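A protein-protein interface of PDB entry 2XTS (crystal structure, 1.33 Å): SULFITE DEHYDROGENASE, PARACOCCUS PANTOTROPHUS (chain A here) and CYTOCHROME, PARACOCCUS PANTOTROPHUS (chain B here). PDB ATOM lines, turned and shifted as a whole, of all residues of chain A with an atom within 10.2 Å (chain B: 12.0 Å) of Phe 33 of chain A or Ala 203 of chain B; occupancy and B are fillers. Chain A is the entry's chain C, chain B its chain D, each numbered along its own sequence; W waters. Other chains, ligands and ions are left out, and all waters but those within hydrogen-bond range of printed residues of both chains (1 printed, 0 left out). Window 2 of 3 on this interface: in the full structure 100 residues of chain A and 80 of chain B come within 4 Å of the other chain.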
ATOM      1  N   LEU A   7       1.486  10.174 -21.164  1.00  0.00           N
ATOM      2  CA  LEU A   7       1.537   9.081 -20.166  1.00  0.00           C
ATOM      3  C   LEU A   7       2.860   9.057 -19.398  1.00  0.00           C
ATOM      4  O   LEU A   7       2.987   8.371 -18.375  1.00  0.00           O
ATOM      5  CB  LEU A   7       1.261   7.708 -20.792  1.00  0.00           C
ATOM      6  CG  LEU A   7      -0.217   7.357 -20.931  1.00  0.00           C
ATOM      7  CD1 LEU A   7      -0.390   6.232 -21.897  1.00  0.00           C
ATOM      8  CD2 LEU A   7      -0.870   7.007 -19.588  1.00  0.00           C
ATOM      9  N   TRP A  14      -1.886   7.051 -10.388  1.00  0.00           N
ATOM     10  CA  TRP A  14      -1.230   5.939  -9.715  1.00  0.00           C
ATOM     11  C   TRP A  14       0.169   6.268  -9.226  1.00  0.00           C
ATOM     12  O   TRP A  14       0.735   5.513  -8.434  1.00  0.00           O
ATOM     13  CB  TRP A  14      -1.231   4.712 -10.612  1.00  0.00           C
ATOM     14  CG  TRP A  14      -0.581   4.877 -11.948  1.00  0.00           C
ATOM     15  CD1 TRP A  14       0.745   4.770 -12.260  1.00  0.00           C
ATOM     16  CD2 TRP A  14      -1.258   5.121 -13.175  1.00  0.00           C
ATOM     17  NE1 TRP A  14       0.930   4.949 -13.612  1.00  0.00           N
ATOM     18  CE2 TRP A  14      -0.289   5.177 -14.192  1.00  0.00           C
ATOM     19  CE3 TRP A  14      -2.590   5.371 -13.513  1.00  0.00           C
ATOM     20  CZ2 TRP A  14      -0.618   5.444 -15.535  1.00  0.00           C
ATOM     21  CZ3 TRP A  14      -2.921   5.612 -14.873  1.00  0.00           C
ATOM     22  CH2 TRP A  14      -1.934   5.641 -15.852  1.00  0.00           C
ATOM     23  N   LEU A  29      -8.055 -12.451  -6.907  1.00  0.00           N
ATOM     24  CA  LEU A  29      -8.311 -12.871  -8.278  1.00  0.00           C
ATOM     25  C   LEU A  29      -7.504 -12.013  -9.252  1.00  0.00           C
ATOM     26  O   LEU A  29      -6.980 -10.990  -8.854  1.00  0.00           O
ATOM     27  CB  LEU A  29      -9.792 -12.682  -8.596  1.00  0.00           C
ATOM     28  CG  LEU A  29     -10.708 -13.768  -8.021  1.00  0.00           C
ATOM     29  CD1 LEU A  29     -12.168 -13.382  -8.102  1.00  0.00           C
ATOM     30  CD2 LEU A  29     -10.459 -15.144  -8.695  1.00  0.00           C
ATOM     31  N   PRO A  30      -7.403 -12.422 -10.528  1.00  0.00           N
ATOM     32  CA  PRO A  30      -6.741 -11.612 -11.534  1.00  0.00           C
ATOM     33  C   PRO A  30      -7.320 -10.221 -11.685  1.00  0.00           C
ATOM     34  O   PRO A  30      -8.503  -9.964 -11.419  1.00  0.00           O
ATOM     35  CB  PRO A  30      -6.986 -12.398 -12.821  1.00  0.00           C
ATOM     36  CG  PRO A  30      -7.053 -13.847 -12.371  1.00  0.00           C
ATOM     37  CD  PRO A  30      -7.798 -13.728 -11.065  1.00  0.00           C
ATOM     38  N   ILE A  31      -6.469  -9.306 -12.125  1.00  0.00           N
ATOM     39  CA  ILE A  31      -6.923  -7.960 -12.449  1.00  0.00           C
ATOM     40  C   ILE A  31      -7.979  -8.055 -13.545  1.00  0.00           C
ATOM     41  O   ILE A  31      -7.953  -8.948 -14.370  1.00  0.00           O
ATOM     42  CB  ILE A  31      -5.717  -7.049 -12.820  1.00  0.00           C
ATOM     43  CG1 ILE A  31      -6.043  -5.564 -12.646  1.00  0.00           C
ATOM     44  CG2 ILE A  31      -5.139  -7.385 -14.192  1.00  0.00           C
ATOM     45  CD1 ILE A  31      -4.795  -4.657 -12.764  1.00  0.00           C
ATOM     46  N   HIS A  32      -8.888  -7.095 -13.580  1.00  0.00           N
ATOM     47  CA  HIS A  32     -10.017  -7.182 -14.505  1.00  0.00           C
ATOM     48  C   HIS A  32      -9.627  -7.123 -15.977  1.00  0.00           C
ATOM     49  O   HIS A  32     -10.345  -7.642 -16.822  1.00  0.00           O
ATOM     50  CB  HIS A  32     -11.094  -6.140 -14.168  1.00  0.00           C
ATOM     51  CG  HIS A  32     -10.704  -4.730 -14.466  1.00  0.00           C
ATOM     52  ND1 HIS A  32     -10.939  -4.133 -15.686  1.00  0.00           N
ATOM     53  CD2 HIS A  32     -10.099  -3.799 -13.698  1.00  0.00           C
ATOM     54  CE1 HIS A  32     -10.506  -2.886 -15.652  1.00  0.00           C
ATOM     55  NE2 HIS A  32      -9.975  -2.665 -14.462  1.00  0.00           N
ATOM     56  N   PHE A  33      -8.483  -6.528 -16.272  1.00  0.00           N
ATOM     57  CA  PHE A  33      -8.010  -6.468 -17.634  1.00  0.00           C
ATOM     58  C   PHE A  33      -7.672  -7.844 -18.194  1.00  0.00           C
ATOM     59  O   PHE A  33      -7.444  -7.996 -19.415  1.00  0.00           O
ATOM     60  CB  PHE A  33      -6.758  -5.596 -17.770  1.00  0.00           C
ATOM     61  CG  PHE A  33      -6.877  -4.202 -17.240  1.00  0.00           C
ATOM     62  CD1 PHE A  33      -7.751  -3.283 -17.820  1.00  0.00           C
ATOM     63  CD2 PHE A  33      -6.077  -3.809 -16.197  1.00  0.00           C
ATOM     64  CE1 PHE A  33      -7.804  -1.992 -17.352  1.00  0.00           C
ATOM     65  CE2 PHE A  33      -6.135  -2.543 -15.723  1.00  0.00           C
ATOM     66  CZ  PHE A  33      -7.002  -1.630 -16.286  1.00  0.00           C
ATOM     67  N   GLU A  34      -7.543  -8.835 -17.308  1.00  0.00           N
ATOM     68  CA  GLU A  34      -7.224 -10.199 -17.711  1.00  0.00           C
ATOM     69  C   GLU A  34      -8.433 -11.129 -17.767  1.00  0.00           C
ATOM     70  O   GLU A  34      -8.323 -12.356 -17.713  1.00  0.00           O
ATOM     71  CB  GLU A  34      -6.140 -10.756 -16.784  1.00  0.00           C
ATOM     72  CG  GLU A  34      -4.816  -9.979 -16.904  1.00  0.00           C
ATOM     73  CD  GLU A  34      -4.178 -10.088 -18.290  1.00  0.00           C
ATOM     74  OE1 GLU A  34      -4.087 -11.235 -18.782  1.00  0.00           O
ATOM     75  OE2 GLU A  34      -3.748  -9.049 -18.868  1.00  0.00           O
ATOM     76  N   SER A  35      -9.602 -10.549 -17.973  1.00  0.00           N
ATOM     77  CA  SER A  35     -10.865 -11.326 -17.891  1.00  0.00           C
ATOM     78  C   SER A  35     -10.995 -12.411 -18.973  1.00  0.00           C
ATOM     79  O   SER A  35     -11.693 -13.389 -18.765  1.00  0.00           O
ATOM     80  CB  SER A  35     -12.063 -10.380 -17.916  1.00  0.00           C
ATOM     81  OG  SER A  35     -12.126  -9.740 -19.172  1.00  0.00           O
ATOM     82  N   HIS A  36     -10.291 -12.237 -20.085  1.00  0.00           N
ATOM     83  CA  HIS A  36     -10.304 -13.206 -21.184  1.00  0.00           C
ATOM     84  C   HIS A  36      -9.532 -14.486 -20.847  1.00  0.00           C
ATOM     85  O   HIS A  36      -9.612 -15.474 -21.574  1.00  0.00           O
ATOM     86  CB  HIS A  36      -9.721 -12.586 -22.460  1.00  0.00           C
ATOM     87  CG  HIS A  36      -8.339 -12.054 -22.267  1.00  0.00           C
ATOM     88  ND1 HIS A  36      -8.086 -10.888 -21.580  1.00  0.00           N
ATOM     89  CD2 HIS A  36      -7.130 -12.550 -22.622  1.00  0.00           C
ATOM     90  CE1 HIS A  36      -6.784 -10.688 -21.519  1.00  0.00           C
ATOM     91  NE2 HIS A  36      -6.178 -11.685 -22.137  1.00  0.00           N
ATOM     92  N   VAL A  37      -8.749 -14.475 -19.774  1.00  0.00           N
ATOM     93  CA  VAL A  37      -7.986 -15.633 -19.354  1.00  0.00           C
ATOM     94  C   VAL A  37      -8.874 -16.392 -18.373  1.00  0.00           C
ATOM     95  O   VAL A  37      -8.764 -16.246 -17.171  1.00  0.00           O
ATOM     96  CB  VAL A  37      -6.601 -15.235 -18.810  1.00  0.00           C
ATOM     97  CG1 VAL A  37      -5.805 -16.489 -18.485  1.00  0.00           C
ATOM     98  CG2 VAL A  37      -5.850 -14.342 -19.819  1.00  0.00           C
ATOM     99  N   LYS A  38      -9.755 -17.213 -18.936  1.00  0.00           N
ATOM    100  CA  LYS A  38     -10.782 -17.910 -18.174  1.00  0.00           C
ATOM    101  C   LYS A  38     -11.148 -19.185 -18.909  1.00  0.00           C
ATOM    102  O   LYS A  38     -10.775 -19.376 -20.057  1.00  0.00           O
ATOM    103  CB  LYS A  38     -12.042 -17.043 -18.006  1.00  0.00           C
ATOM    104  CG  LYS A  38     -12.683 -16.607 -19.299  1.00  0.00           C
ATOM    105  CD  LYS A  38     -13.906 -15.731 -19.046  1.00  0.00           C
ATOM    106  CE  LYS A  38     -14.456 -15.234 -20.343  1.00  0.00           C
ATOM    107  NZ  LYS A  38     -15.724 -14.505 -20.139  1.00  0.00           N
ATOM    108  N   ALA A  60      -3.314 -17.908 -23.765  1.00  0.00           N
ATOM    109  CA  ALA A  60      -2.934 -16.712 -23.023  1.00  0.00           C
ATOM    110  C   ALA A  60      -1.926 -16.972 -21.931  1.00  0.00           C
ATOM    111  O   ALA A  60      -1.333 -16.023 -21.414  1.00  0.00           O
ATOM    112  CB  ALA A  60      -4.182 -16.037 -22.390  1.00  0.00           C
ATOM    113  N   ASP B 187     -16.547 -13.670 -29.022  1.00  0.00           N
ATOM    114  CA  ASP B 187     -16.631 -12.389 -28.316  1.00  0.00           C
ATOM    115  C   ASP B 187     -17.637 -11.481 -29.067  1.00  0.00           C
ATOM    116  O   ASP B 187     -18.013 -11.782 -30.210  1.00  0.00           O
ATOM    117  CB  ASP B 187     -15.269 -11.678 -28.343  1.00  0.00           C
ATOM    118  CG  ASP B 187     -14.204 -12.284 -27.403  1.00  0.00           C
ATOM    119  OD1 ASP B 187     -14.552 -13.015 -26.447  1.00  0.00           O
ATOM    120  OD2 ASP B 187     -12.997 -12.011 -27.680  1.00  0.00           O
ATOM    121  N   GLY B 194     -12.534 -15.208 -25.911  1.00  0.00           N
ATOM    122  CA  GLY B 194     -11.287 -15.189 -25.167  1.00  0.00           C
ATOM    123  C   GLY B 194     -10.106 -14.616 -25.922  1.00  0.00           C
ATOM    124  O   GLY B 194      -8.994 -14.633 -25.430  1.00  0.00           O
ATOM    125  N   SER B 195     -10.347 -14.060 -27.105  1.00  0.00           N
ATOM    126  CA  SER B 195      -9.273 -13.456 -27.886  1.00  0.00           C
ATOM    127  C   SER B 195      -8.585 -12.343 -27.099  1.00  0.00           C
ATOM    128  O   SER B 195      -9.202 -11.624 -26.327  1.00  0.00           O
ATOM    129  CB  SER B 195      -9.829 -12.931 -29.223  1.00  0.00           C
ATOM    130  OG  SER B 195     -10.086 -14.007 -30.104  1.00  0.00           O
ATOM    131  N   MET B 196      -7.296 -12.202 -27.335  1.00  0.00           N
ATOM    132  CA  MET B 196      -6.517 -11.227 -26.598  1.00  0.00           C
ATOM    133  C   MET B 196      -6.994  -9.800 -26.921  1.00  0.00           C
ATOM    134  O   MET B 196      -7.254  -9.466 -28.075  1.00  0.00           O
ATOM    135  CB  MET B 196      -5.026 -11.378 -26.924  1.00  0.00           C
ATOM    136  CG  MET B 196      -4.465 -12.796 -26.764  1.00  0.00           C
ATOM    137  SD  MET B 196      -4.356 -13.401 -25.068  1.00  0.00           S
ATOM    138  CE  MET B 196      -3.074 -12.329 -24.405  1.00  0.00           C
ATOM    139  N   PRO B 197      -7.083  -8.954 -25.898  1.00  0.00           N
ATOM    140  CA  PRO B 197      -7.427  -7.569 -26.160  1.00  0.00           C
ATOM    141  C   PRO B 197      -6.394  -6.872 -27.052  1.00  0.00           C
ATOM    142  O   PRO B 197      -5.195  -7.141 -26.972  1.00  0.00           O
ATOM    143  CB  PRO B 197      -7.406  -6.937 -24.768  1.00  0.00           C
ATOM    144  CG  PRO B 197      -7.514  -8.039 -23.799  1.00  0.00           C
ATOM    145  CD  PRO B 197      -6.961  -9.243 -24.456  1.00  0.00           C
ATOM    146  N   ASP B 198      -6.889  -5.978 -27.901  1.00  0.00           N
ATOM    147  CA  ASP B 198      -6.031  -5.142 -28.722  1.00  0.00           C
ATOM    148  C   ASP B 198      -5.391  -4.071 -27.853  1.00  0.00           C
ATOM    149  O   ASP B 198      -6.071  -3.180 -27.350  1.00  0.00           O
ATOM    150  CB  ASP B 198      -6.885  -4.515 -29.827  1.00  0.00           C
ATOM    151  CG  ASP B 198      -6.082  -3.664 -30.809  1.00  0.00           C
ATOM    152  OD1 ASP B 198      -4.848  -3.519 -30.673  1.00  0.00           O
ATOM    153  OD2 ASP B 198      -6.720  -3.113 -31.739  1.00  0.00           O
ATOM    154  N   LEU B 199      -4.084  -4.159 -27.656  1.00  0.00           N
ATOM    155  CA  LEU B 199      -3.387  -3.171 -26.836  1.00  0.00           C
ATOM    156  C   LEU B 199      -3.276  -1.796 -27.527  1.00  0.00           C
ATOM    157  O   LEU B 199      -2.944  -0.797 -26.879  1.00  0.00           O
ATOM    158  CB  LEU B 199      -2.028  -3.732 -26.390  1.00  0.00           C
ATOM    159  CG  LEU B 199      -2.128  -5.019 -25.545  1.00  0.00           C
ATOM    160  CD1 LEU B 199      -0.777  -5.476 -25.029  1.00  0.00           C
ATOM    161  CD2 LEU B 199      -3.113  -4.857 -24.375  1.00  0.00           C
ATOM    162  N   GLY B 200      -3.561  -1.742 -28.827  1.00  0.00           N
ATOM    163  CA  GLY B 200      -3.662  -0.475 -29.551  1.00  0.00           C
ATOM    164  C   GLY B 200      -4.999   0.231 -29.363  1.00  0.00           C
ATOM    165  O   GLY B 200      -5.137   1.399 -29.757  1.00  0.00           O
ATOM    166  N   ALA B 201      -5.980  -0.445 -28.765  1.00  0.00           N
ATOM    167  CA  ALA B 201      -7.274   0.142 -28.431  1.00  0.00           C
ATOM    168  C   ALA B 201      -7.353   0.413 -26.940  1.00  0.00           C
ATOM    169  O   ALA B 201      -6.535  -0.093 -26.166  1.00  0.00           O
ATOM    170  CB  ALA B 201      -8.402  -0.785 -28.856  1.00  0.00           C
ATOM    171  N   ALA B 202      -8.339   1.206 -26.539  1.00  0.00           N
ATOM    172  CA  ALA B 202      -8.508   1.576 -25.143  1.00  0.00           C
ATOM    173  C   ALA B 202      -8.777   0.342 -24.282  1.00  0.00           C
ATOM    174  O   ALA B 202      -9.389  -0.632 -24.736  1.00  0.00           O
ATOM    175  CB  ALA B 202      -9.640   2.584 -24.992  1.00  0.00           C
ATOM    176  N   ALA B 203      -8.296   0.404 -23.044  1.00  0.00           N
ATOM    177  CA  ALA B 203      -8.495  -0.645 -22.051  1.00  0.00           C
ATOM    178  C   ALA B 203      -9.954  -0.688 -21.613  1.00  0.00           C
ATOM    179  O   ALA B 203     -10.627   0.343 -21.554  1.00  0.00           O
ATOM    180  CB  ALA B 203      -7.604  -0.384 -20.838  1.00  0.00           C
ATOM    181  N   ALA B 204     -10.431  -1.887 -21.293  1.00  0.00           N
ATOM    182  CA  ALA B 204     -11.820  -2.083 -20.889  1.00  0.00           C
ATOM    183  C   ALA B 204     -12.100  -1.470 -19.521  1.00  0.00           C
ATOM    184  O   ALA B 204     -11.223  -1.441 -18.654  1.00  0.00           O
ATOM    185  CB  ALA B 204     -12.150  -3.572 -20.865  1.00  0.00           C
ATOM    186  N   PRO B 205     -13.326  -0.981 -19.345  1.00  0.00           N
ATOM    187  CA  PRO B 205     -13.824  -0.549 -18.043  1.00  0.00           C
ATOM    188  C   PRO B 205     -13.941  -1.757 -17.119  1.00  0.00           C
ATOM    189  O   PRO B 205     -13.787  -1.668 -15.900  1.00  0.00           O
ATOM    190  CB  PRO B 205     -15.180   0.118 -18.194  1.00  0.00           C
ATOM    191  OXT PRO B 205     -14.201  -2.864 -17.590  1.00  0.00           O
HETATM  192  O   HOH W   1     -12.811  -5.463 -17.405  1.00  0.00           O
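OD1 of Asp 187 of chain B is in hydrogen-bond range of N of Gly 194 of chain B, at 3.0 Å.
His 32 of chain A touches Ala 204 of chain B (CE1 to O, 3.4 Å). Pro 205 of chain B touches His 32 of chain A. Ala 203 of chain B touches Phe 33 of chain A (CB to CE1, 3.8 Å). Ala 204 of chain B touches Phe 33 of chain A. Gly 194 of chain B touches His 36 of chain A. His 36 of chain A touches Met 196 of chain B (CD2 to SD, 3.8 Å). His 36 of chain A touches Pro 197 of chain B. Ala 60 of chain A touches Met 196 of chain B (CB to SD, 3.8 Å).
Phe 33 of chain A touches just these residues of chain B: Ala 203 and Ala 204. Of the printed residues of chain A, Ala 203 of chain B touches Phe 33 (3.8 Å). Ile 31 of chain A touches none of the printed residues of chain B. His 32 of chain A touches just these residues of chain B: Ala 204 (3.4 Å) and Pro 205 (3.5 Å). No residue of chain B comes within 4 Å of Glu 34 of chain A. No residue of chain A comes within 4 Å of Ala 202 of chain B. Of the printed residues of chain A, Gly 194 of chain B touches His 36. Of the printed residues of chain A, Pro 197 of chain B touches His 36. Of the printed residues of chain A, Pro 205 of chain B touches His 32. Asp 198 of chain B touches none of the printed residues of chain A. Leu 199 of chain B touches none of the printed residues of chain A. The nearest residue of chain B that does not touch Phe 33 of chain A is Pro 197 of chain B (4.4 Å). The nearest residue of chain A that does not touch Ala 203 of chain B is His 32 of chain A (6.4 Å).
Of the 13 printed residues of chain B, 6 touch a printed residue of chain A. Of the 13 printed residues of chain A, 4 touch a printed residue of chain B. Hydrophobic or aromatic side chains of chain A within 4 Å of the printed part of chain B: His 32, Phe 33, His 36 and Ala 60. Among the printed residues, 8 pairs touch across the chains. Among the printed residues, no Asp or Glu carboxylate lies within 4 Å of a Lys or Arg side-chain nitrogen of the other chain.
Water W1 lies within hydrogen-bond range of ND1 of His 32 of chain A and OXT of Pro 205 of chain B.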
